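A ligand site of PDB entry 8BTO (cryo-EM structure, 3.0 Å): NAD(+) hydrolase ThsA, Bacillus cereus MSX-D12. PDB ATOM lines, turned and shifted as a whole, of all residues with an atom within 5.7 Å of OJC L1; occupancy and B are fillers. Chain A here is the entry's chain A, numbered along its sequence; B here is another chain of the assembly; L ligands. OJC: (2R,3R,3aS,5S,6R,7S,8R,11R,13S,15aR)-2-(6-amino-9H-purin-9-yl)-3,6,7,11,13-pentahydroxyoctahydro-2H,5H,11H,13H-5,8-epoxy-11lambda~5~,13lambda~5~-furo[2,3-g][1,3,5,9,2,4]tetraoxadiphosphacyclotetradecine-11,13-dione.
N of Asn 390 sits at hydrogen-bond distance from O of Ser 293 (2.9 Å).
NE2 of Gln 362 lies within hydrogen-bond range of O of Phe 360 (3.3 Å).
The backbone NH of Phe 327 of chain A sits close to the side-chain hydroxyl of Ser 325, at 3.4 Å.
The side-chain hydroxyl (OG) of Ser 291 is in hydrogen-bond range of the side-chain carboxylate (OE1) of Glu 406 (2.5 Å).
The side-chain carboxylate (OE2) of Glu 406 lies within salt-bridge range of the guanidinium group (NE) of Arg 374 (3.1 Å).
Residues that only touch OJC L1: Gly 326 (3.7 Å), Phe 327 of chain A (3.8 Å), Gly 328 (3.3 Å), Phe 360 (3.5 Å), Trp 370 (3.3 Å), Ala 400 (3.3 Å) and Lys 401 (3.6 Å).
Hydrophobic or aromatic side chains within 4 Å of OJC L1: Leu 329, Phe 360, Trp 370, Ala 400 and Val 403.
17 residues have an atom within 4 Å of OJC L1: Ser 291, Gly 292, Ser 293, Gly 326, Phe 327 of chain A, Gly 328, Leu 329, Phe 360, Gln 362, Trp 370, Arg 374, Lys 391, Ala 400, Lys 401, Gly 402, Val 403 and Glu 406.
NZ of Lys 391 lies within salt-bridge range of O5 of OJC L1 (3.4 Å).
The backbone NH (N) of Gly 292 is in hydrogen-bond range of an oxygen (O11) of OJC L1 (2.9 Å).
An oxygen (O10) of OJC L1 is in hydrogen-bond range of the side-chain carboxylate (OE2) of Glu 406 (2.6 Å).
OG of Ser 293 sits at hydrogen-bond distance from O6 of OJC L1 (3.0 Å).
N of Gly 402 lies within hydrogen-bond range of O5 of OJC L1 (2.7 Å).
The side-chain hydroxyl of Ser 291 is in hydrogen-bond range of an oxygen (O11) of OJC L1 (3.5 Å).
The backbone NH (N) of Val 403 is in hydrogen-bond range of an oxygen (O7) of OJC L1 (3.5 Å).
The guanidinium group (NH2) of Arg 374 is in hydrogen-bond range of an oxygen (O8) of OJC L1 (2.7 Å).
The backbone NH of Leu 329 lies within hydrogen-bond range of an oxygen (O12) of OJC L1, at 2.7 Å.
An oxygen (O) of OJC L1 is in hydrogen-bond range of the side-chain amide nitrogen of Gln 362.
O of Gly 292 sits at hydrogen-bond distance from O11 of OJC L1.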
ATOM      1  N   PHE A 289     -30.134  -9.190 -24.758  1.00  0.00           N
ATOM      2  CA  PHE A 289     -29.798 -10.601 -24.648  1.00  0.00           C
ATOM      3  C   PHE A 289     -28.645 -10.896 -25.603  1.00  0.00           C
ATOM      4  O   PHE A 289     -28.853 -10.971 -26.822  1.00  0.00           O
ATOM      5  CB  PHE A 289     -31.006 -11.486 -24.956  1.00  0.00           C
ATOM      6  CG  PHE A 289     -30.722 -12.950 -24.862  1.00  0.00           C
ATOM      7  CD1 PHE A 289     -30.589 -13.570 -23.635  1.00  0.00           C
ATOM      8  CD2 PHE A 289     -30.594 -13.721 -26.013  1.00  0.00           C
ATOM      9  CE1 PHE A 289     -30.320 -14.912 -23.549  1.00  0.00           C
ATOM     10  CE2 PHE A 289     -30.331 -15.071 -25.925  1.00  0.00           C
ATOM     11  CZ  PHE A 289     -30.193 -15.666 -24.687  1.00  0.00           C
ATOM     12  N   LEU A 290     -27.452 -11.061 -25.056  1.00  0.00           N
ATOM     13  CA  LEU A 290     -26.256 -11.331 -25.854  1.00  0.00           C
ATOM     14  C   LEU A 290     -26.223 -12.827 -26.160  1.00  0.00           C
ATOM     15  O   LEU A 290     -25.780 -13.649 -25.350  1.00  0.00           O
ATOM     16  CB  LEU A 290     -24.993 -10.887 -25.122  1.00  0.00           C
ATOM     17  CG  LEU A 290     -24.914  -9.391 -24.855  1.00  0.00           C
ATOM     18  CD1 LEU A 290     -23.568  -9.016 -24.269  1.00  0.00           C
ATOM     19  CD2 LEU A 290     -25.185  -8.617 -26.130  1.00  0.00           C
ATOM     20  N   SER A 291     -26.691 -13.181 -27.354  1.00  0.00           N
ATOM     21  CA  SER A 291     -26.708 -14.568 -27.791  1.00  0.00           C
ATOM     22  C   SER A 291     -25.516 -14.856 -28.682  1.00  0.00           C
ATOM     23  O   SER A 291     -25.068 -13.992 -29.444  1.00  0.00           O
ATOM     24  CB  SER A 291     -28.003 -14.889 -28.528  1.00  0.00           C
ATOM     25  OG  SER A 291     -27.969 -16.205 -29.051  1.00  0.00           O
ATOM     26  N   GLY A 292     -25.006 -16.070 -28.582  1.00  0.00           N
ATOM     27  CA  GLY A 292     -23.903 -16.472 -29.427  1.00  0.00           C
ATOM     28  C   GLY A 292     -23.118 -17.603 -28.797  1.00  0.00           C
ATOM     29  O   GLY A 292     -23.239 -17.911 -27.620  1.00  0.00           O
ATOM     30  N   SER A 293     -22.281 -18.227 -29.632  1.00  0.00           N
ATOM     31  CA  SER A 293     -21.402 -19.307 -29.235  1.00  0.00           C
ATOM     32  C   SER A 293     -20.378 -19.493 -30.332  1.00  0.00           C
ATOM     33  O   SER A 293     -20.744 -19.566 -31.509  1.00  0.00           O
ATOM     34  CB  SER A 293     -22.191 -20.604 -28.997  1.00  0.00           C
ATOM     35  OG  SER A 293     -22.794 -21.069 -30.194  1.00  0.00           O
ATOM     36  N   SER A 325     -27.141 -13.140 -20.255  1.00  0.00           N
ATOM     37  CA  SER A 325     -26.315 -14.043 -21.042  1.00  0.00           C
ATOM     38  C   SER A 325     -26.575 -15.484 -20.611  1.00  0.00           C
ATOM     39  O   SER A 325     -26.664 -15.761 -19.413  1.00  0.00           O
ATOM     40  CB  SER A 325     -24.832 -13.706 -20.905  1.00  0.00           C
ATOM     41  OG  SER A 325     -24.039 -14.504 -21.775  1.00  0.00           O
ATOM     42  N   GLY A 326     -26.699 -16.369 -21.586  1.00  0.00           N
ATOM     43  CA  GLY A 326     -26.829 -17.786 -21.315  1.00  0.00           C
ATOM     44  C   GLY A 326     -25.516 -18.495 -21.049  1.00  0.00           C
ATOM     45  O   GLY A 326     -25.492 -19.730 -20.979  1.00  0.00           O
ATOM     46  N   PHE A 327     -24.437 -17.736 -20.897  1.00  0.00           N
ATOM     47  CA  PHE A 327     -23.096 -18.292 -20.680  1.00  0.00           C
ATOM     48  C   PHE A 327     -22.732 -19.267 -21.796  1.00  0.00           C
ATOM     49  O   PHE A 327     -22.253 -20.377 -21.548  1.00  0.00           O
ATOM     50  CB  PHE A 327     -22.986 -18.936 -19.296  1.00  0.00           C
ATOM     51  CG  PHE A 327     -21.570 -19.194 -18.867  1.00  0.00           C
ATOM     52  CD1 PHE A 327     -20.694 -18.142 -18.652  1.00  0.00           C
ATOM     53  CD2 PHE A 327     -21.118 -20.481 -18.658  1.00  0.00           C
ATOM     54  CE1 PHE A 327     -19.401 -18.379 -18.256  1.00  0.00           C
ATOM     55  CE2 PHE A 327     -19.825 -20.730 -18.254  1.00  0.00           C
ATOM     56  CZ  PHE A 327     -18.958 -19.674 -18.058  1.00  0.00           C
ATOM     57  N   GLY A 328     -22.971 -18.852 -23.027  1.00  0.00           N
ATOM     58  CA  GLY A 328     -22.633 -19.673 -24.165  1.00  0.00           C
ATOM     59  C   GLY A 328     -21.137 -19.820 -24.346  1.00  0.00           C
ATOM     60  O   GLY A 328     -20.344 -18.965 -23.953  1.00  0.00           O
ATOM     61  N   LEU A 329     -20.748 -20.930 -24.956  1.00  0.00           N
ATOM     62  CA  LEU A 329     -19.326 -21.229 -25.136  1.00  0.00           C
ATOM     63  C   LEU A 329     -18.720 -20.282 -26.161  1.00  0.00           C
ATOM     64  O   LEU A 329     -19.060 -20.326 -27.345  1.00  0.00           O
ATOM     65  CB  LEU A 329     -19.138 -22.678 -25.579  1.00  0.00           C
ATOM     66  CG  LEU A 329     -18.990 -23.725 -24.478  1.00  0.00           C
ATOM     67  CD1 LEU A 329     -18.724 -25.091 -25.079  1.00  0.00           C
ATOM     68  CD2 LEU A 329     -17.882 -23.333 -23.513  1.00  0.00           C
ATOM     69  N   VAL A 331     -18.622 -16.763 -25.933  1.00  0.00           N
ATOM     70  CA  VAL A 331     -19.006 -15.371 -25.785  1.00  0.00           C
ATOM     71  C   VAL A 331     -19.379 -15.073 -24.336  1.00  0.00           C
ATOM     72  O   VAL A 331     -19.242 -13.939 -23.873  1.00  0.00           O
ATOM     73  CB  VAL A 331     -20.171 -14.996 -26.722  1.00  0.00           C
ATOM     74  CG1 VAL A 331     -19.830 -15.371 -28.161  1.00  0.00           C
ATOM     75  CG2 VAL A 331     -21.446 -15.654 -26.277  1.00  0.00           C
ATOM     76  N   PHE A 360     -26.378 -22.994 -18.977  1.00  0.00           N
ATOM     77  CA  PHE A 360     -27.254 -24.097 -19.350  1.00  0.00           C
ATOM     78  C   PHE A 360     -26.780 -25.395 -18.702  1.00  0.00           C
ATOM     79  O   PHE A 360     -25.611 -25.765 -18.875  1.00  0.00           O
ATOM     80  CB  PHE A 360     -27.312 -24.255 -20.867  1.00  0.00           C
ATOM     81  CG  PHE A 360     -28.327 -23.361 -21.525  1.00  0.00           C
ATOM     82  CD1 PHE A 360     -28.043 -22.024 -21.725  1.00  0.00           C
ATOM     83  CD2 PHE A 360     -29.531 -23.867 -21.949  1.00  0.00           C
ATOM     84  CE1 PHE A 360     -28.974 -21.207 -22.333  1.00  0.00           C
ATOM     85  CE2 PHE A 360     -30.462 -23.050 -22.556  1.00  0.00           C
ATOM     86  CZ  PHE A 360     -30.172 -21.717 -22.751  1.00  0.00           C
ATOM     87  N   GLN A 362     -25.595 -28.926 -18.200  1.00  0.00           N
ATOM     88  CA  GLN A 362     -25.036 -29.897 -19.128  1.00  0.00           C
ATOM     89  C   GLN A 362     -25.400 -31.306 -18.675  1.00  0.00           C
ATOM     90  O   GLN A 362     -25.183 -31.678 -17.520  1.00  0.00           O
ATOM     91  CB  GLN A 362     -23.526 -29.735 -19.222  1.00  0.00           C
ATOM     92  CG  GLN A 362     -23.088 -28.397 -19.812  1.00  0.00           C
ATOM     93  CD  GLN A 362     -23.593 -28.196 -21.230  1.00  0.00           C
ATOM     94  OE1 GLN A 362     -23.620 -29.127 -22.029  1.00  0.00           O
ATOM     95  NE2 GLN A 362     -24.006 -26.971 -21.547  1.00  0.00           N
ATOM     96  N   TRP A 370     -33.997 -27.360 -21.196  1.00  0.00           N
ATOM     97  CA  TRP A 370     -33.296 -26.290 -21.914  1.00  0.00           C
ATOM     98  C   TRP A 370     -34.257 -25.330 -22.615  1.00  0.00           C
ATOM     99  O   TRP A 370     -34.032 -24.126 -22.616  1.00  0.00           O
ATOM    100  CB  TRP A 370     -32.333 -26.884 -22.953  1.00  0.00           C
ATOM    101  CG  TRP A 370     -30.965 -27.147 -22.441  1.00  0.00           C
ATOM    102  CD1 TRP A 370     -30.516 -26.963 -21.171  1.00  0.00           C
ATOM    103  CD2 TRP A 370     -29.859 -27.638 -23.190  1.00  0.00           C
ATOM    104  NE1 TRP A 370     -29.192 -27.314 -21.081  1.00  0.00           N
ATOM    105  CE2 TRP A 370     -28.758 -27.737 -22.306  1.00  0.00           C
ATOM    106  CE3 TRP A 370     -29.674 -28.012 -24.521  1.00  0.00           C
ATOM    107  CZ2 TRP A 370     -27.506 -28.181 -22.712  1.00  0.00           C
ATOM    108  CZ3 TRP A 370     -28.429 -28.464 -24.924  1.00  0.00           C
ATOM    109  CH2 TRP A 370     -27.361 -28.540 -24.020  1.00  0.00           C
ATOM    110  N   ARG A 374     -34.529 -21.423 -21.812  1.00  0.00           N
ATOM    111  CA  ARG A 374     -34.185 -20.397 -22.804  1.00  0.00           C
ATOM    112  C   ARG A 374     -35.310 -19.435 -23.019  1.00  0.00           C
ATOM    113  O   ARG A 374     -35.080 -18.269 -23.223  1.00  0.00           O
ATOM    114  CB  ARG A 374     -33.872 -21.110 -24.100  1.00  0.00           C
ATOM    115  CG  ARG A 374     -33.386 -20.264 -25.254  1.00  0.00           C
ATOM    116  CD  ARG A 374     -32.831 -21.181 -26.321  1.00  0.00           C
ATOM    117  NE  ARG A 374     -31.404 -21.411 -26.135  1.00  0.00           N
ATOM    118  CZ  ARG A 374     -30.773 -22.507 -26.516  1.00  0.00           C
ATOM    119  NH1 ARG A 374     -31.437 -23.493 -27.085  1.00  0.00           N
ATOM    120  NH2 ARG A 374     -29.475 -22.617 -26.314  1.00  0.00           N
ATOM    121  N   MET A 377     -35.150 -17.085 -20.056  1.00  0.00           N
ATOM    122  CA  MET A 377     -34.088 -16.102 -20.234  1.00  0.00           C
ATOM    123  C   MET A 377     -34.523 -14.994 -21.188  1.00  0.00           C
ATOM    124  O   MET A 377     -34.438 -13.804 -20.860  1.00  0.00           O
ATOM    125  CB  MET A 377     -32.820 -16.761 -20.787  1.00  0.00           C
ATOM    126  CG  MET A 377     -32.214 -17.838 -19.917  1.00  0.00           C
ATOM    127  SD  MET A 377     -30.693 -18.453 -20.651  1.00  0.00           S
ATOM    128  CE  MET A 377     -31.081 -18.337 -22.381  1.00  0.00           C
ATOM    129  N   ASN A 390     -21.343 -20.667 -34.103  1.00  0.00           N
ATOM    130  CA  ASN A 390     -20.872 -21.992 -34.498  1.00  0.00           C
ATOM    131  C   ASN A 390     -20.477 -22.793 -33.265  1.00  0.00           C
ATOM    132  O   ASN A 390     -20.269 -22.257 -32.179  1.00  0.00           O
ATOM    133  CB  ASN A 390     -19.713 -21.891 -35.490  1.00  0.00           C
ATOM    134  CG  ASN A 390     -18.593 -21.020 -34.996  1.00  0.00           C
ATOM    135  OD1 ASN A 390     -18.572 -20.612 -33.835  1.00  0.00           O
ATOM    136  ND2 ASN A 390     -17.643 -20.716 -35.870  1.00  0.00           N
ATOM    137  N   LYS A 391     -20.405 -24.069 -33.363  1.00  0.00           N
ATOM    138  CA  LYS A 391     -20.034 -24.916 -32.239  1.00  0.00           C
ATOM    139  C   LYS A 391     -19.331 -26.143 -32.782  1.00  0.00           C
ATOM    140  O   LYS A 391     -19.606 -26.569 -33.894  1.00  0.00           O
ATOM    141  CB  LYS A 391     -21.250 -25.352 -31.438  1.00  0.00           C
ATOM    142  CG  LYS A 391     -22.172 -26.350 -32.116  1.00  0.00           C
ATOM    143  CD  LYS A 391     -23.304 -26.723 -31.192  1.00  0.00           C
ATOM    144  CE  LYS A 391     -24.355 -27.559 -31.906  1.00  0.00           C
ATOM    145  NZ  LYS A 391     -25.612 -27.662 -31.123  1.00  0.00           N
ATOM    146  N   ALA A 400     -24.235 -23.682 -34.921  1.00  0.00           N
ATOM    147  CA  ALA A 400     -24.936 -23.942 -33.668  1.00  0.00           C
ATOM    148  C   ALA A 400     -26.409 -23.581 -33.820  1.00  0.00           C
ATOM    149  O   ALA A 400     -26.739 -22.409 -34.052  1.00  0.00           O
ATOM    150  CB  ALA A 400     -24.290 -23.149 -32.537  1.00  0.00           C
ATOM    151  N   LYS A 401     -27.287 -24.566 -33.646  1.00  0.00           N
ATOM    152  CA  LYS A 401     -28.718 -24.337 -33.794  1.00  0.00           C
ATOM    153  C   LYS A 401     -29.346 -23.625 -32.602  1.00  0.00           C
ATOM    154  O   LYS A 401     -30.481 -23.163 -32.716  1.00  0.00           O
ATOM    155  CB  LYS A 401     -29.430 -25.678 -34.027  1.00  0.00           C
ATOM    156  N   GLY A 402     -28.643 -23.539 -31.471  1.00  0.00           N
ATOM    157  CA  GLY A 402     -29.180 -22.825 -30.328  1.00  0.00           C
ATOM    158  C   GLY A 402     -29.321 -21.336 -30.578  1.00  0.00           C
ATOM    159  O   GLY A 402     -30.254 -20.707 -30.084  1.00  0.00           O
ATOM    160  N   VAL A 403     -28.388 -20.754 -31.322  1.00  0.00           N
ATOM    161  CA  VAL A 403     -28.516 -19.343 -31.680  1.00  0.00           C
ATOM    162  C   VAL A 403     -29.750 -19.120 -32.539  1.00  0.00           C
ATOM    163  O   VAL A 403     -30.492 -18.146 -32.346  1.00  0.00           O
ATOM    164  CB  VAL A 403     -27.240 -18.842 -32.381  1.00  0.00           C
ATOM    165  CG1 VAL A 403     -27.315 -17.351 -32.602  1.00  0.00           C
ATOM    166  CG2 VAL A 403     -26.014 -19.191 -31.559  1.00  0.00           C
ATOM    167  N   GLU A 406     -32.759 -19.306 -30.293  1.00  0.00           N
ATOM    168  CA  GLU A 406     -32.919 -18.096 -29.542  1.00  0.00           C
ATOM    169  C   GLU A 406     -33.498 -17.019 -30.426  1.00  0.00           C
ATOM    170  O   GLU A 406     -34.420 -16.338 -30.023  1.00  0.00           O
ATOM    171  CB  GLU A 406     -31.589 -17.665 -28.962  1.00  0.00           C
ATOM    172  CG  GLU A 406     -31.353 -18.265 -27.600  1.00  0.00           C
ATOM    173  CD  GLU A 406     -29.899 -18.490 -27.290  1.00  0.00           C
ATOM    174  OE1 GLU A 406     -29.061 -18.322 -28.178  1.00  0.00           O
ATOM    175  OE2 GLU A 406     -29.612 -18.871 -26.136  1.00  0.00           O
ATOM    176  N   PHE B 327     -21.445 -22.182 -10.490  1.00  0.00           N
ATOM    177  CA  PHE B 327     -21.479 -23.035 -11.675  1.00  0.00           C
ATOM    178  C   PHE B 327     -20.190 -23.840 -11.792  1.00  0.00           C
ATOM    179  O   PHE B 327     -19.568 -23.917 -12.862  1.00  0.00           O
ATOM    180  CB  PHE B 327     -21.753 -22.214 -12.943  1.00  0.00           C
ATOM    181  CG  PHE B 327     -22.154 -23.050 -14.127  1.00  0.00           C
ATOM    182  CD1 PHE B 327     -23.334 -23.761 -14.114  1.00  0.00           C
ATOM    183  CD2 PHE B 327     -21.361 -23.090 -15.258  1.00  0.00           C
ATOM    184  CE1 PHE B 327     -23.714 -24.522 -15.197  1.00  0.00           C
ATOM    185  CE2 PHE B 327     -21.732 -23.849 -16.350  1.00  0.00           C
ATOM    186  CZ  PHE B 327     -22.908 -24.571 -16.316  1.00  0.00           C
HETATM  187  N   OJC L   1     -19.885 -25.523 -20.305  1.00  0.00           N
HETATM  188  C   OJC L   1     -20.688 -24.447 -20.320  1.00  0.00           C
HETATM  189  O   OJC L   1     -24.646 -24.482 -23.334  1.00  0.00           O
HETATM  190  C1  OJC L   1     -19.924 -26.401 -21.335  1.00  0.00           C
HETATM  191  C2  OJC L   1     -20.832 -26.142 -22.362  1.00  0.00           C
HETATM  192  C3  OJC L   1     -21.605 -25.009 -22.248  1.00  0.00           C
HETATM  193  C10 OJC L   1     -25.683 -21.299 -28.248  1.00  0.00           C
HETATM  194  C11 OJC L   1     -26.504 -20.562 -27.224  1.00  0.00           C
HETATM  195  C12 OJC L   1     -25.776 -19.470 -26.427  1.00  0.00           C
HETATM  196  C13 OJC L   1     -26.251 -19.702 -25.001  1.00  0.00           C
HETATM  197  C14 OJC L   1     -26.365 -21.208 -24.984  1.00  0.00           C
HETATM  198  C4  OJC L   1     -22.052 -26.084 -24.101  1.00  0.00           C
HETATM  199  C5  OJC L   1     -23.393 -23.976 -23.703  1.00  0.00           C
HETATM  200  C6  OJC L   1     -23.511 -23.705 -25.195  1.00  0.00           C
HETATM  201  C7  OJC L   1     -24.920 -23.118 -25.245  1.00  0.00           C
HETATM  202  C8  OJC L   1     -25.671 -23.942 -24.200  1.00  0.00           C
HETATM  203  C9  OJC L   1     -26.527 -25.051 -24.751  1.00  0.00           C
HETATM  204  N1  OJC L   1     -21.588 -24.117 -21.249  1.00  0.00           N
HETATM  205  N2  OJC L   1     -22.394 -24.977 -23.379  1.00  0.00           N
HETATM  206  N3  OJC L   1     -21.129 -26.808 -23.531  1.00  0.00           N
HETATM  207  N4  OJC L   1     -19.115 -27.463 -21.300  1.00  0.00           N
HETATM  208  O1  OJC L   1     -25.750 -25.888 -25.616  1.00  0.00           O
HETATM  209  O10 OJC L   1     -27.493 -19.077 -24.720  1.00  0.00           O
HETATM  210  O11 OJC L   1     -26.033 -18.168 -26.926  1.00  0.00           O
HETATM  211  O12 OJC L   1     -22.521 -22.846 -25.707  1.00  0.00           O
HETATM  212  O2  OJC L   1     -27.531 -26.339 -27.306  1.00  0.00           O
HETATM  213  O3  OJC L   1     -25.057 -26.742 -27.846  1.00  0.00           O
HETATM  214  O4  OJC L   1     -25.992 -24.439 -27.683  1.00  0.00           O
HETATM  215  O5  OJC L   1     -26.504 -24.497 -30.096  1.00  0.00           O
HETATM  216  O6  OJC L   1     -24.309 -23.471 -29.252  1.00  0.00           O
HETATM  217  O7  OJC L   1     -26.478 -22.306 -28.888  1.00  0.00           O
HETATM  218  O8  OJC L   1     -26.983 -21.493 -26.227  1.00  0.00           O
HETATM  219  O9  OJC L   1     -25.057 -21.745 -24.934  1.00  0.00           O
HETATM  220  P   OJC L   1     -26.113 -25.945 -27.171  1.00  0.00           P
HETATM  221  P1  OJC L   1     -25.756 -23.715 -29.089  1.00  0.00           P
HETATM  222  N   OJC L   2     -16.782 -24.324 -17.936  1.00  0.00           N
HETATM  223  C   OJC L   2     -17.417 -23.849 -16.849  1.00  0.00           C
HETATM  224  O   OJC L   2     -14.697 -22.481 -12.916  1.00  0.00           O
HETATM  225  C1  OJC L   2     -15.513 -24.770 -17.823  1.00  0.00           C
HETATM  226  C2  OJC L   2     -14.919 -24.691 -16.559  1.00  0.00           C
HETATM  227  C3  OJC L   2     -15.674 -24.176 -15.527  1.00  0.00           C
HETATM  228  C10 OJC L   2     -14.267 -25.011  -7.552  1.00  0.00           C
HETATM  229  C11 OJC L   2     -15.200 -23.860  -7.280  1.00  0.00           C
HETATM  230  C12 OJC L   2     -16.692 -24.128  -7.505  1.00  0.00           C
HETATM  231  C13 OJC L   2     -17.164 -22.876  -8.224  1.00  0.00           C
HETATM  232  C14 OJC L   2     -15.942 -22.562  -9.057  1.00  0.00           C
HETATM  233  C4  OJC L   2     -13.685 -24.763 -14.829  1.00  0.00           C
HETATM  234  C5  OJC L   2     -15.225 -23.766 -13.076  1.00  0.00           C
HETATM  235  C6  OJC L   2     -14.597 -24.587 -11.967  1.00  0.00           C
HETATM  236  C7  OJC L   2     -14.665 -23.585 -10.823  1.00  0.00           C
HETATM  237  C8  OJC L   2     -14.382 -22.255 -11.516  1.00  0.00           C
HETATM  238  C9  OJC L   2     -12.979 -21.734 -11.368  1.00  0.00           C
HETATM  239  N1  OJC L   2     -16.930 -23.733 -15.606  1.00  0.00           N
HETATM  240  N2  OJC L   2     -14.878 -24.218 -14.412  1.00  0.00           N
HETATM  241  N3  OJC L   2     -13.665 -25.055 -16.098  1.00  0.00           N
HETATM  242  N4  OJC L   2     -14.898 -25.238 -18.898  1.00  0.00           N
HETATM  243  O1  OJC L   2     -12.055 -22.745 -11.774  1.00  0.00           O
HETATM  244  O10 OJC L   2     -17.484 -21.818  -7.345  1.00  0.00           O
HETATM  245  O11 OJC L   2     -17.378 -24.397  -6.292  1.00  0.00           O
HETATM  246  O12 OJC L   2     -15.261 -25.799 -11.701  1.00  0.00           O
HETATM  247  O2  OJC L   2     -10.292 -22.262 -10.074  1.00  0.00           O
HETATM  248  O3  OJC L   2     -10.323 -24.488 -11.337  1.00  0.00           O
HETATM  249  O4  OJC L   2     -11.999 -23.980  -9.572  1.00  0.00           O
HETATM  250  O5  OJC L   2     -10.499 -24.999  -7.887  1.00  0.00           O
HETATM  251  O6  OJC L   2     -12.351 -26.380  -8.983  1.00  0.00           O
HETATM  252  O7  OJC L   2     -12.907 -24.612  -7.332  1.00  0.00           O
HETATM  253  O8  OJC L   2     -14.880 -22.757  -8.154  1.00  0.00           O
HETATM  254  O9  OJC L   2     -15.890 -23.491 -10.127  1.00  0.00           O
HETATM  255  P   OJC L   2     -11.049 -23.367 -10.697  1.00  0.00           P
HETATM  256  P1  OJC L   2     -11.867 -25.102  -8.442  1.00  0.00           P
